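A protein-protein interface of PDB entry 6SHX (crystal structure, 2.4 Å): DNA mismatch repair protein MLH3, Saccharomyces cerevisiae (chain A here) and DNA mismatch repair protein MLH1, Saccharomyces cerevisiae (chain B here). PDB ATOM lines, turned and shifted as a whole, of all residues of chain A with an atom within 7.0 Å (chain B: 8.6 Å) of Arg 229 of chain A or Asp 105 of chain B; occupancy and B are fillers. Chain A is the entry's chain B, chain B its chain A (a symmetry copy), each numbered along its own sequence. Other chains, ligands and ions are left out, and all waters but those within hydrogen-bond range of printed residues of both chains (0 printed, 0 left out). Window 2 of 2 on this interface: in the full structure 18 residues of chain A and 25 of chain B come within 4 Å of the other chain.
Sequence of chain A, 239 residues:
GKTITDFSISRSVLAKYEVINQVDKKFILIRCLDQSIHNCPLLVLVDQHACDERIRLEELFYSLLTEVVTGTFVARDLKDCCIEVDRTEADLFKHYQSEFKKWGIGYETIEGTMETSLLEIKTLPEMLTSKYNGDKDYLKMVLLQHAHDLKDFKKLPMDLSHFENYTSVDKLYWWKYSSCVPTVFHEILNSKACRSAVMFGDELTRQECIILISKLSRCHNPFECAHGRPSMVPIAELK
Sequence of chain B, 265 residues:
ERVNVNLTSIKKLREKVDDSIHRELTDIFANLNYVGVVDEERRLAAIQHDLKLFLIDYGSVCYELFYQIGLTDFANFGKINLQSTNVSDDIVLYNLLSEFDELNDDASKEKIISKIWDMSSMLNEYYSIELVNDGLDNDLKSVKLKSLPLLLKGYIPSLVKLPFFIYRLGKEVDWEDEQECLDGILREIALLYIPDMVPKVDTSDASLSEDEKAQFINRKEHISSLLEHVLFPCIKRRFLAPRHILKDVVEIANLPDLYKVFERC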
ATOM      1  N   ALA A  50      12.905  16.326 -38.466  1.00  0.00           N
ATOM      2  CA  ALA A  50      13.414  15.156 -37.736  1.00  0.00           C
ATOM      3  C   ALA A  50      12.519  13.924 -37.936  1.00  0.00           C
ATOM      4  O   ALA A  50      13.033  12.835 -38.188  1.00  0.00           O
ATOM      5  CB  ALA A  50      13.540  15.477 -36.254  1.00  0.00           C
ATOM      6  N   PHE A 223      12.212   8.382 -31.620  1.00  0.00           N
ATOM      7  CA  PHE A 223      12.588   9.458 -30.705  1.00  0.00           C
ATOM      8  C   PHE A 223      13.839  10.255 -31.081  1.00  0.00           C
ATOM      9  O   PHE A 223      14.159  11.223 -30.384  1.00  0.00           O
ATOM     10  CB  PHE A 223      12.691   8.914 -29.279  1.00  0.00           C
ATOM     11  CG  PHE A 223      11.450   8.145 -28.892  1.00  0.00           C
ATOM     12  CD1 PHE A 223      10.245   8.804 -28.671  1.00  0.00           C
ATOM     13  CD2 PHE A 223      11.471   6.759 -28.810  1.00  0.00           C
ATOM     14  CE1 PHE A 223       9.087   8.087 -28.351  1.00  0.00           C
ATOM     15  CE2 PHE A 223      10.316   6.045 -28.480  1.00  0.00           C
ATOM     16  CZ  PHE A 223       9.131   6.715 -28.252  1.00  0.00           C
ATOM     17  N   GLU A 224      14.497   9.924 -32.197  1.00  0.00           N
ATOM     18  CA  GLU A 224      15.642  10.718 -32.636  1.00  0.00           C
ATOM     19  C   GLU A 224      15.678  10.911 -34.150  1.00  0.00           C
ATOM     20  O   GLU A 224      15.017  10.177 -34.877  1.00  0.00           O
ATOM     21  CB  GLU A 224      16.979  10.182 -32.089  1.00  0.00           C
ATOM     22  CG  GLU A 224      17.563   8.997 -32.831  1.00  0.00           C
ATOM     23  CD  GLU A 224      18.974   8.632 -32.417  1.00  0.00           C
ATOM     24  OE1 GLU A 224      19.207   8.428 -31.204  1.00  0.00           O
ATOM     25  OE2 GLU A 224      19.846   8.537 -33.312  1.00  0.00           O
ATOM     26  N   CYS A 225      16.439  11.906 -34.617  1.00  0.00           N
ATOM     27  CA  CYS A 225      16.608  12.187 -36.041  1.00  0.00           C
ATOM     28  C   CYS A 225      17.757  11.304 -36.576  1.00  0.00           C
ATOM     29  O   CYS A 225      18.198  10.390 -35.870  1.00  0.00           O
ATOM     30  CB  CYS A 225      16.877  13.676 -36.259  1.00  0.00           C
ATOM     31  SG  CYS A 225      18.403  14.284 -35.488  1.00  0.00           S
ATOM     32  N   ALA A 226      18.252  11.570 -37.797  1.00  0.00           N
ATOM     33  CA  ALA A 226      19.377  10.818 -38.363  1.00  0.00           C
ATOM     34  C   ALA A 226      20.731  11.200 -37.722  1.00  0.00           C
ATOM     35  O   ALA A 226      21.711  10.480 -37.921  1.00  0.00           O
ATOM     36  CB  ALA A 226      19.434  11.004 -39.877  1.00  0.00           C
ATOM     37  N   HIS A 227      20.782  12.300 -36.939  1.00  0.00           N
ATOM     38  CA  HIS A 227      22.016  12.792 -36.323  1.00  0.00           C
ATOM     39  C   HIS A 227      22.026  12.753 -34.781  1.00  0.00           C
ATOM     40  O   HIS A 227      22.629  13.622 -34.152  1.00  0.00           O
ATOM     41  CB  HIS A 227      22.341  14.194 -36.852  1.00  0.00           C
ATOM     42  CG  HIS A 227      22.346  14.252 -38.343  1.00  0.00           C
ATOM     43  ND1 HIS A 227      21.197  14.558 -39.054  1.00  0.00           N
ATOM     44  CD2 HIS A 227      23.338  13.962 -39.217  1.00  0.00           C
ATOM     45  CE1 HIS A 227      21.534  14.483 -40.331  1.00  0.00           C
ATOM     46  NE2 HIS A 227      22.811  14.125 -40.480  1.00  0.00           N
ATOM     47  N   GLY A 228      21.404  11.724 -34.204  1.00  0.00           N
ATOM     48  CA  GLY A 228      21.358  11.478 -32.763  1.00  0.00           C
ATOM     49  C   GLY A 228      20.808  12.568 -31.860  1.00  0.00           C
ATOM     50  O   GLY A 228      21.198  12.656 -30.693  1.00  0.00           O
ATOM     51  N   ARG A 229      19.907  13.403 -32.383  1.00  0.00           N
ATOM     52  CA  ARG A 229      19.262  14.483 -31.635  1.00  0.00           C
ATOM     53  C   ARG A 229      17.756  14.178 -31.531  1.00  0.00           C
ATOM     54  O   ARG A 229      17.265  13.446 -32.393  1.00  0.00           O
ATOM     55  CB  ARG A 229      19.535  15.838 -32.307  1.00  0.00           C
ATOM     56  CG  ARG A 229      20.749  16.539 -31.723  1.00  0.00           C
ATOM     57  CD  ARG A 229      21.578  17.248 -32.768  1.00  0.00           C
ATOM     58  NE  ARG A 229      22.499  16.334 -33.447  1.00  0.00           N
ATOM     59  CZ  ARG A 229      23.692  16.680 -33.922  1.00  0.00           C
ATOM     60  NH1 ARG A 229      24.133  17.926 -33.789  1.00  0.00           N
ATOM     61  NH2 ARG A 229      24.456  15.782 -34.531  1.00  0.00           N
ATOM     62  N   PRO A 230      17.009  14.659 -30.494  1.00  0.00           N
ATOM     63  CA  PRO A 230      15.575  14.304 -30.391  1.00  0.00           C
ATOM     64  C   PRO A 230      14.704  14.719 -31.574  1.00  0.00           C
ATOM     65  O   PRO A 230      15.022  15.679 -32.280  1.00  0.00           O
ATOM     66  CB  PRO A 230      15.118  14.984 -29.095  1.00  0.00           C
ATOM     67  CG  PRO A 230      16.118  16.031 -28.835  1.00  0.00           C
ATOM     68  CD  PRO A 230      17.423  15.520 -29.367  1.00  0.00           C
ATOM     69  N   SER A 231      13.623  13.959 -31.806  1.00  0.00           N
ATOM     70  CA  SER A 231      12.664  14.213 -32.880  1.00  0.00           C
ATOM     71  C   SER A 231      11.440  14.962 -32.333  1.00  0.00           C
ATOM     72  O   SER A 231      10.680  15.568 -33.092  1.00  0.00           O
ATOM     73  CB  SER A 231      12.218  12.894 -33.498  1.00  0.00           C
ATOM     74  OG  SER A 231      11.599  12.101 -32.500  1.00  0.00           O
ATOM     75  N   MET A 232      11.240  14.878 -31.009  1.00  0.00           N
ATOM     76  CA  MET A 232      10.119  15.470 -30.292  1.00  0.00           C
ATOM     77  C   MET A 232      10.486  15.895 -28.868  1.00  0.00           C
ATOM     78  O   MET A 232      11.441  15.375 -28.292  1.00  0.00           O
ATOM     79  CB  MET A 232       8.905  14.517 -30.298  1.00  0.00           C
ATOM     80  CG  MET A 232       9.123  13.219 -29.539  1.00  0.00           C
ATOM     81  SD  MET A 232       7.831  11.996 -29.846  1.00  0.00           S
ATOM     82  CE  MET A 232       8.276  11.471 -31.477  1.00  0.00           C
ATOM     83  N   TYR B  94      28.463  14.383 -18.589  1.00  0.00           N
ATOM     84  CA  TYR B  94      28.465  15.568 -19.457  1.00  0.00           C
ATOM     85  C   TYR B  94      29.887  16.097 -19.679  1.00  0.00           C
ATOM     86  O   TYR B  94      30.168  16.652 -20.745  1.00  0.00           O
ATOM     87  CB  TYR B  94      27.546  16.671 -18.895  1.00  0.00           C
ATOM     88  CG  TYR B  94      27.230  17.766 -19.892  1.00  0.00           C
ATOM     89  CD1 TYR B  94      26.187  17.629 -20.803  1.00  0.00           C
ATOM     90  CD2 TYR B  94      27.969  18.946 -19.921  1.00  0.00           C
ATOM     91  CE1 TYR B  94      25.899  18.628 -21.732  1.00  0.00           C
ATOM     92  CE2 TYR B  94      27.695  19.950 -20.849  1.00  0.00           C
ATOM     93  CZ  TYR B  94      26.653  19.790 -21.749  1.00  0.00           C
ATOM     94  OH  TYR B  94      26.365  20.781 -22.656  1.00  0.00           O
ATOM     95  N   LEU B  97      31.842  13.543 -22.177  1.00  0.00           N
ATOM     96  CA  LEU B  97      31.432  13.710 -23.574  1.00  0.00           C
ATOM     97  C   LEU B  97      32.006  14.964 -24.246  1.00  0.00           C
ATOM     98  O   LEU B  97      31.845  15.122 -25.458  1.00  0.00           O
ATOM     99  CB  LEU B  97      29.898  13.662 -23.715  1.00  0.00           C
ATOM    100  CG  LEU B  97      29.207  12.330 -23.384  1.00  0.00           C
ATOM    101  CD1 LEU B  97      27.718  12.525 -23.219  1.00  0.00           C
ATOM    102  CD2 LEU B  97      29.484  11.269 -24.443  1.00  0.00           C
ATOM    103  N   PHE B 100      34.639  14.780 -27.399  1.00  0.00           N
ATOM    104  CA  PHE B 100      34.164  14.540 -28.762  1.00  0.00           C
ATOM    105  C   PHE B 100      33.709  15.833 -29.434  1.00  0.00           C
ATOM    106  O   PHE B 100      32.855  16.542 -28.897  1.00  0.00           O
ATOM    107  CB  PHE B 100      33.046  13.476 -28.773  1.00  0.00           C
ATOM    108  CG  PHE B 100      33.350  12.229 -27.974  1.00  0.00           C
ATOM    109  CD1 PHE B 100      34.053  11.175 -28.540  1.00  0.00           C
ATOM    110  CD2 PHE B 100      32.929  12.108 -26.655  1.00  0.00           C
ATOM    111  CE1 PHE B 100      34.339  10.024 -27.799  1.00  0.00           C
ATOM    112  CE2 PHE B 100      33.216  10.958 -25.914  1.00  0.00           C
ATOM    113  CZ  PHE B 100      33.920   9.926 -26.491  1.00  0.00           C
ATOM    114  N   ASP B 101      34.297  16.140 -30.605  1.00  0.00           N
ATOM    115  CA  ASP B 101      33.987  17.341 -31.391  1.00  0.00           C
ATOM    116  C   ASP B 101      32.707  17.188 -32.223  1.00  0.00           C
ATOM    117  O   ASP B 101      32.161  18.184 -32.709  1.00  0.00           O
ATOM    118  CB  ASP B 101      35.187  17.745 -32.263  1.00  0.00           C
ATOM    119  CG  ASP B 101      36.373  18.237 -31.456  1.00  0.00           C
ATOM    120  OD1 ASP B 101      36.303  19.372 -30.930  1.00  0.00           O
ATOM    121  OD2 ASP B 101      37.370  17.490 -31.349  1.00  0.00           O
ATOM    122  N   GLU B 102      32.221  15.935 -32.353  1.00  0.00           N
ATOM    123  CA  GLU B 102      30.994  15.554 -33.062  1.00  0.00           C
ATOM    124  C   GLU B 102      29.762  15.974 -32.241  1.00  0.00           C
ATOM    125  O   GLU B 102      28.679  16.166 -32.803  1.00  0.00           O
ATOM    126  CB  GLU B 102      30.963  14.032 -33.308  1.00  0.00           C
ATOM    127  CG  GLU B 102      32.126  13.503 -34.136  1.00  0.00           C
ATOM    128  CD  GLU B 102      32.820  12.267 -33.590  1.00  0.00           C
ATOM    129  OE1 GLU B 102      32.942  12.141 -32.350  1.00  0.00           O
ATOM    130  OE2 GLU B 102      33.261  11.430 -34.411  1.00  0.00           O
ATOM    131  N   LEU B 103      29.939  16.107 -30.912  1.00  0.00           N
ATOM    132  CA  LEU B 103      28.893  16.497 -29.967  1.00  0.00           C
ATOM    133  C   LEU B 103      29.050  17.969 -29.567  1.00  0.00           C
ATOM    134  O   LEU B 103      29.009  18.313 -28.381  1.00  0.00           O
ATOM    135  CB  LEU B 103      28.907  15.575 -28.730  1.00  0.00           C
ATOM    136  CG  LEU B 103      29.004  14.065 -28.951  1.00  0.00           C
ATOM    137  CD1 LEU B 103      29.176  13.354 -27.636  1.00  0.00           C
ATOM    138  CD2 LEU B 103      27.794  13.527 -29.704  1.00  0.00           C
ATOM    139  N   ASN B 104      29.216  18.833 -30.583  1.00  0.00           N
ATOM    140  CA  ASN B 104      29.390  20.287 -30.480  1.00  0.00           C
ATOM    141  C   ASN B 104      28.230  21.028 -29.780  1.00  0.00           C
ATOM    142  O   ASN B 104      28.462  22.075 -29.172  1.00  0.00           O
ATOM    143  CB  ASN B 104      29.661  20.893 -31.869  1.00  0.00           C
ATOM    144  CG  ASN B 104      28.913  20.229 -33.009  1.00  0.00           C
ATOM    145  OD1 ASN B 104      27.677  20.249 -33.081  1.00  0.00           O
ATOM    146  ND2 ASN B 104      29.652  19.623 -33.926  1.00  0.00           N
ATOM    147  N   ASP B 105      26.999  20.485 -29.864  1.00  0.00           N
ATOM    148  CA  ASP B 105      25.795  21.074 -29.265  1.00  0.00           C
ATOM    149  C   ASP B 105      25.316  20.329 -28.014  1.00  0.00           C
ATOM    150  O   ASP B 105      25.674  19.167 -27.807  1.00  0.00           O
ATOM    151  CB  ASP B 105      24.666  21.171 -30.311  1.00  0.00           C
ATOM    152  CG  ASP B 105      24.259  19.839 -30.913  1.00  0.00           C
ATOM    153  OD1 ASP B 105      25.132  19.154 -31.492  1.00  0.00           O
ATOM    154  OD2 ASP B 105      23.073  19.482 -30.807  1.00  0.00           O
ATOM    155  N   ASP B 106      24.491  21.008 -27.190  1.00  0.00           N
ATOM    156  CA  ASP B 106      23.916  20.464 -25.956  1.00  0.00           C
ATOM    157  C   ASP B 106      22.904  19.349 -26.221  1.00  0.00           C
ATOM    158  O   ASP B 106      22.877  18.376 -25.470  1.00  0.00           O
ATOM    159  CB  ASP B 106      23.289  21.578 -25.099  1.00  0.00           C
ATOM    160  CG  ASP B 106      24.274  22.511 -24.409  1.00  0.00           C
ATOM    161  OD1 ASP B 106      25.495  22.389 -24.662  1.00  0.00           O
ATOM    162  OD2 ASP B 106      23.823  23.366 -23.614  1.00  0.00           O
ATOM    163  N   ALA B 107      22.098  19.480 -27.300  1.00  0.00           N
ATOM    164  CA  ALA B 107      21.077  18.508 -27.713  1.00  0.00           C
ATOM    165  C   ALA B 107      21.662  17.122 -28.012  1.00  0.00           C
ATOM    166  O   ALA B 107      21.106  16.123 -27.557  1.00  0.00           O
ATOM    167  CB  ALA B 107      20.301  19.033 -28.912  1.00  0.00           C
ATOM    168  N   SER B 108      22.797  17.069 -28.739  1.00  0.00           N
ATOM    169  CA  SER B 108      23.492  15.828 -29.090  1.00  0.00           C
ATOM    170  C   SER B 108      24.058  15.105 -27.858  1.00  0.00           C
ATOM    171  O   SER B 108      23.885  13.888 -27.747  1.00  0.00           O
ATOM    172  CB  SER B 108      24.585  16.087 -30.126  1.00  0.00           C
ATOM    173  OG  SER B 108      25.493  17.093 -29.710  1.00  0.00           O
ATOM    174  N   LYS B 109      24.709  15.859 -26.931  1.00  0.00           N
ATOM    175  CA  LYS B 109      25.293  15.348 -25.678  1.00  0.00           C
ATOM    176  C   LYS B 109      24.198  14.863 -24.718  1.00  0.00           C
ATOM    177  O   LYS B 109      24.311  13.769 -24.163  1.00  0.00           O
ATOM    178  CB  LYS B 109      26.126  16.441 -24.976  1.00  0.00           C
ATOM    179  CG  LYS B 109      27.561  16.581 -25.450  1.00  0.00           C
ATOM    180  CD  LYS B 109      28.276  17.651 -24.640  1.00  0.00           C
ATOM    181  CE  LYS B 109      29.707  17.863 -25.057  1.00  0.00           C
ATOM    182  NZ  LYS B 109      30.357  18.913 -24.231  1.00  0.00           N
ATOM    183  N   GLU B 110      23.145  15.689 -24.522  1.00  0.00           N
ATOM    184  CA  GLU B 110      22.024  15.390 -23.630  1.00  0.00           C
ATOM    185  C   GLU B 110      21.182  14.203 -24.082  1.00  0.00           C
ATOM    186  O   GLU B 110      20.605  13.534 -23.227  1.00  0.00           O
ATOM    187  CB  GLU B 110      21.150  16.624 -23.396  1.00  0.00           C
ATOM    188  CG  GLU B 110      21.731  17.572 -22.363  1.00  0.00           C
ATOM    189  CD  GLU B 110      21.047  18.921 -22.283  1.00  0.00           C
ATOM    190  OE1 GLU B 110      21.704  19.932 -22.618  1.00  0.00           O
ATOM    191  OE2 GLU B 110      19.861  18.970 -21.885  1.00  0.00           O
ATOM    192  N   LYS B 111      21.122  13.932 -25.408  1.00  0.00           N
ATOM    193  CA  LYS B 111      20.379  12.801 -25.971  1.00  0.00           C
ATOM    194  C   LYS B 111      21.005  11.488 -25.521  1.00  0.00           C
ATOM    195  O   LYS B 111      20.281  10.542 -25.212  1.00  0.00           O
ATOM    196  CB  LYS B 111      20.348  12.865 -27.507  1.00  0.00           C
ATOM    197  CG  LYS B 111      19.025  12.404 -28.113  1.00  0.00           C
ATOM    198  CD  LYS B 111      18.927  10.890 -28.331  1.00  0.00           C
ATOM    199  CE  LYS B 111      17.494  10.427 -28.478  1.00  0.00           C
ATOM    200  NZ  LYS B 111      16.735  10.494 -27.199  1.00  0.00           N
ATOM    201  N   ILE B 112      22.351  11.439 -25.478  1.00  0.00           N
ATOM    202  CA  ILE B 112      23.137  10.283 -25.045  1.00  0.00           C
ATOM    203  C   ILE B 112      22.862  10.014 -23.559  1.00  0.00           C
ATOM    204  O   ILE B 112      22.457   8.902 -23.212  1.00  0.00           O
ATOM    205  CB  ILE B 112      24.651  10.479 -25.377  1.00  0.00           C
ATOM    206  CG1 ILE B 112      24.871  10.475 -26.907  1.00  0.00           C
ATOM    207  CG2 ILE B 112      25.530   9.414 -24.693  1.00  0.00           C
ATOM    208  CD1 ILE B 112      26.021  11.255 -27.377  1.00  0.00           C
ATOM    209  N   LYS B 115      19.151   8.741 -22.834  1.00  0.00           N
ATOM    210  CA  LYS B 115      18.975   7.325 -23.183  1.00  0.00           C
ATOM    211  C   LYS B 115      19.451   6.419 -22.047  1.00  0.00           C
ATOM    212  O   LYS B 115      18.744   5.483 -21.669  1.00  0.00           O
ATOM    213  CB  LYS B 115      19.736   6.984 -24.475  1.00  0.00           C
ATOM    214  CG  LYS B 115      19.057   7.432 -25.758  1.00  0.00           C
ATOM    215  CD  LYS B 115      19.979   7.199 -26.938  1.00  0.00           C
ATOM    216  CE  LYS B 115      19.240   6.799 -28.187  1.00  0.00           C
ATOM    217  NZ  LYS B 115      20.138   6.100 -29.143  1.00  0.00           N
ATOM    218  N   LYS B 141      22.988  17.516 -16.753  1.00  0.00           N
ATOM    219  CA  LYS B 141      24.334  18.056 -16.551  1.00  0.00           C
ATOM    220  C   LYS B 141      24.999  17.575 -15.252  1.00  0.00           C
ATOM    221  O   LYS B 141      26.228  17.599 -15.164  1.00  0.00           O
ATOM    222  CB  LYS B 141      24.312  19.591 -16.613  1.00  0.00           C
ATOM    223  CG  LYS B 141      24.431  20.142 -18.025  1.00  0.00           C
ATOM    224  CD  LYS B 141      23.114  20.702 -18.535  1.00  0.00           C
ATOM    225  CE  LYS B 141      23.255  21.311 -19.909  1.00  0.00           C
ATOM    226  NZ  LYS B 141      24.001  22.598 -19.882  1.00  0.00           N
ATOM    227  N   TYR B 167      29.666   7.298 -24.508  1.00  0.00           N
ATOM    228  CA  TYR B 167      29.367   7.745 -25.867  1.00  0.00           C
ATOM    229  C   TYR B 167      28.700   6.626 -26.672  1.00  0.00           C
ATOM    230  O   TYR B 167      27.650   6.847 -27.271  1.00  0.00           O
ATOM    231  CB  TYR B 167      30.665   8.208 -26.554  1.00  0.00           C
ATOM    232  CG  TYR B 167      30.499   8.740 -27.962  1.00  0.00           C
ATOM    233  CD1 TYR B 167      29.549   9.715 -28.253  1.00  0.00           C
ATOM    234  CD2 TYR B 167      31.345   8.329 -28.986  1.00  0.00           C
ATOM    235  CE1 TYR B 167      29.413  10.230 -29.542  1.00  0.00           C
ATOM    236  CE2 TYR B 167      31.227   8.848 -30.275  1.00  0.00           C
ATOM    237  CZ  TYR B 167      30.263   9.806 -30.548  1.00  0.00           C
ATOM    238  OH  TYR B 167      30.135  10.325 -31.815  1.00  0.00           O
ATOM    239  N   LYS B 171      24.896   6.282 -28.345  1.00  0.00           N
ATOM    240  CA  LYS B 171      24.958   6.271 -29.809  1.00  0.00           C
ATOM    241  C   LYS B 171      24.936   4.864 -30.455  1.00  0.00           C
ATOM    242  O   LYS B 171      24.240   4.687 -31.457  1.00  0.00           O
ATOM    243  CB  LYS B 171      26.189   7.064 -30.290  1.00  0.00           C
ATOM    244  CG  LYS B 171      26.111   7.547 -31.734  1.00  0.00           C
ATOM    245  CD  LYS B 171      27.485   7.928 -32.268  1.00  0.00           C
ATOM    246  CE  LYS B 171      27.494   8.080 -33.769  1.00  0.00           C
ATOM    247  NZ  LYS B 171      28.877   8.137 -34.305  1.00  0.00           N
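Hydrophobic or aromatic side chains of chain B that line the printed part of chain A: Ala 107.
Hydrophobic or aromatic side chains of chain A that line the printed part of chain B: Pro 230.
Among the printed residues, 8 pairs touch across the chains.
Among the printed residues, Asp or Glu carboxylates within 4 Å of a Lys or Arg side-chain nitrogen of the other chain: Glu 224 of chain A with Lys 115 of chain B (3.2 Å) and Arg 229 of chain A with Asp 105 of chain B (2.8 Å).
CE of Lys 111 of chain B touches O of Phe 223 of chain A, at 3.9 Å.
Lys 111 of chain B touches Glu 224 of chain A.
Gly 228 of chain A touches Lys 111 of chain B (O to CB, 3.3 Å).
CG of Arg 229 of chain A touches CB of Ala 107 of chain B (3.8 Å).
N of Ser 108 of chain B touches CG of Arg 229 of chain A, at 3.7 Å.
Pro 230 of chain A touches Lys 111 of chain B (CD to CG, 3.7 Å).
The side-chain carboxylate of Glu 224 of chain A lies within salt-bridge range of the side-chain amino group of Lys 115 of chain B (3.2 Å).
NH1 of Arg 229 of chain A is in salt-bridge range of OD1 of Asp 105 of chain B.
Of the printed residues of chain B, Phe 223 of chain A touches Lys 111.
Of the printed residues of chain B, Glu 224 of chain A touches Lys 111 (3.7 Å) and Lys 115 (3.2 Å).
Gly 228 of chain A touches one residue of chain B.
Of chain B, only Asp 105 (2.8 Å), Ala 107 (3.8 Å) and Ser 108 (3.7 Å) come within 4 Å of Arg 229 of chain A.
Pro 230 of chain A touches just one residue of chain B: Lys 111 (3.7 Å).
Of the printed residues of chain A, Asp 105 of chain B touches Arg 229 (2.8 Å).
Of the printed residues of chain A, Ala 107 of chain B touches Arg 229 (3.8 Å).
Tyr 167 of chain B touches none of the printed residues of chain A.
The nearest residue of chain B that does not touch Arg 229 of chain A is Lys 111 of chain B (4.1 Å).
The nearest printed residue of chain A that does not touch Ser 108 of chain B is Gly 228 of chain A (4.2 Å).
The side-chain carboxylate (OD1) of Asp 105 of chain B lies within hydrogen-bond range of the side-chain hydroxyl (OG) of Ser 108 of chain B (2.7 Å).
OD1 of Asn 104 of chain B sits close to OD1 of Asp 105 of chain B (3.2 Å).
The backbone carbonyl oxygen (O) of His 227 of chain A lies within hydrogen-bond range of the guanidinium group (NE) of Arg 229 of chain A (2.8 Å).
SG of Cys 225 of chain A sits at hydrogen-bond distance from O of Arg 229 of chain A.
The backbone NH of Ser 231 of chain A lies within hydrogen-bond range of the backbone carbonyl oxygen of Phe 223 of chain A, 3.1 Å away.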
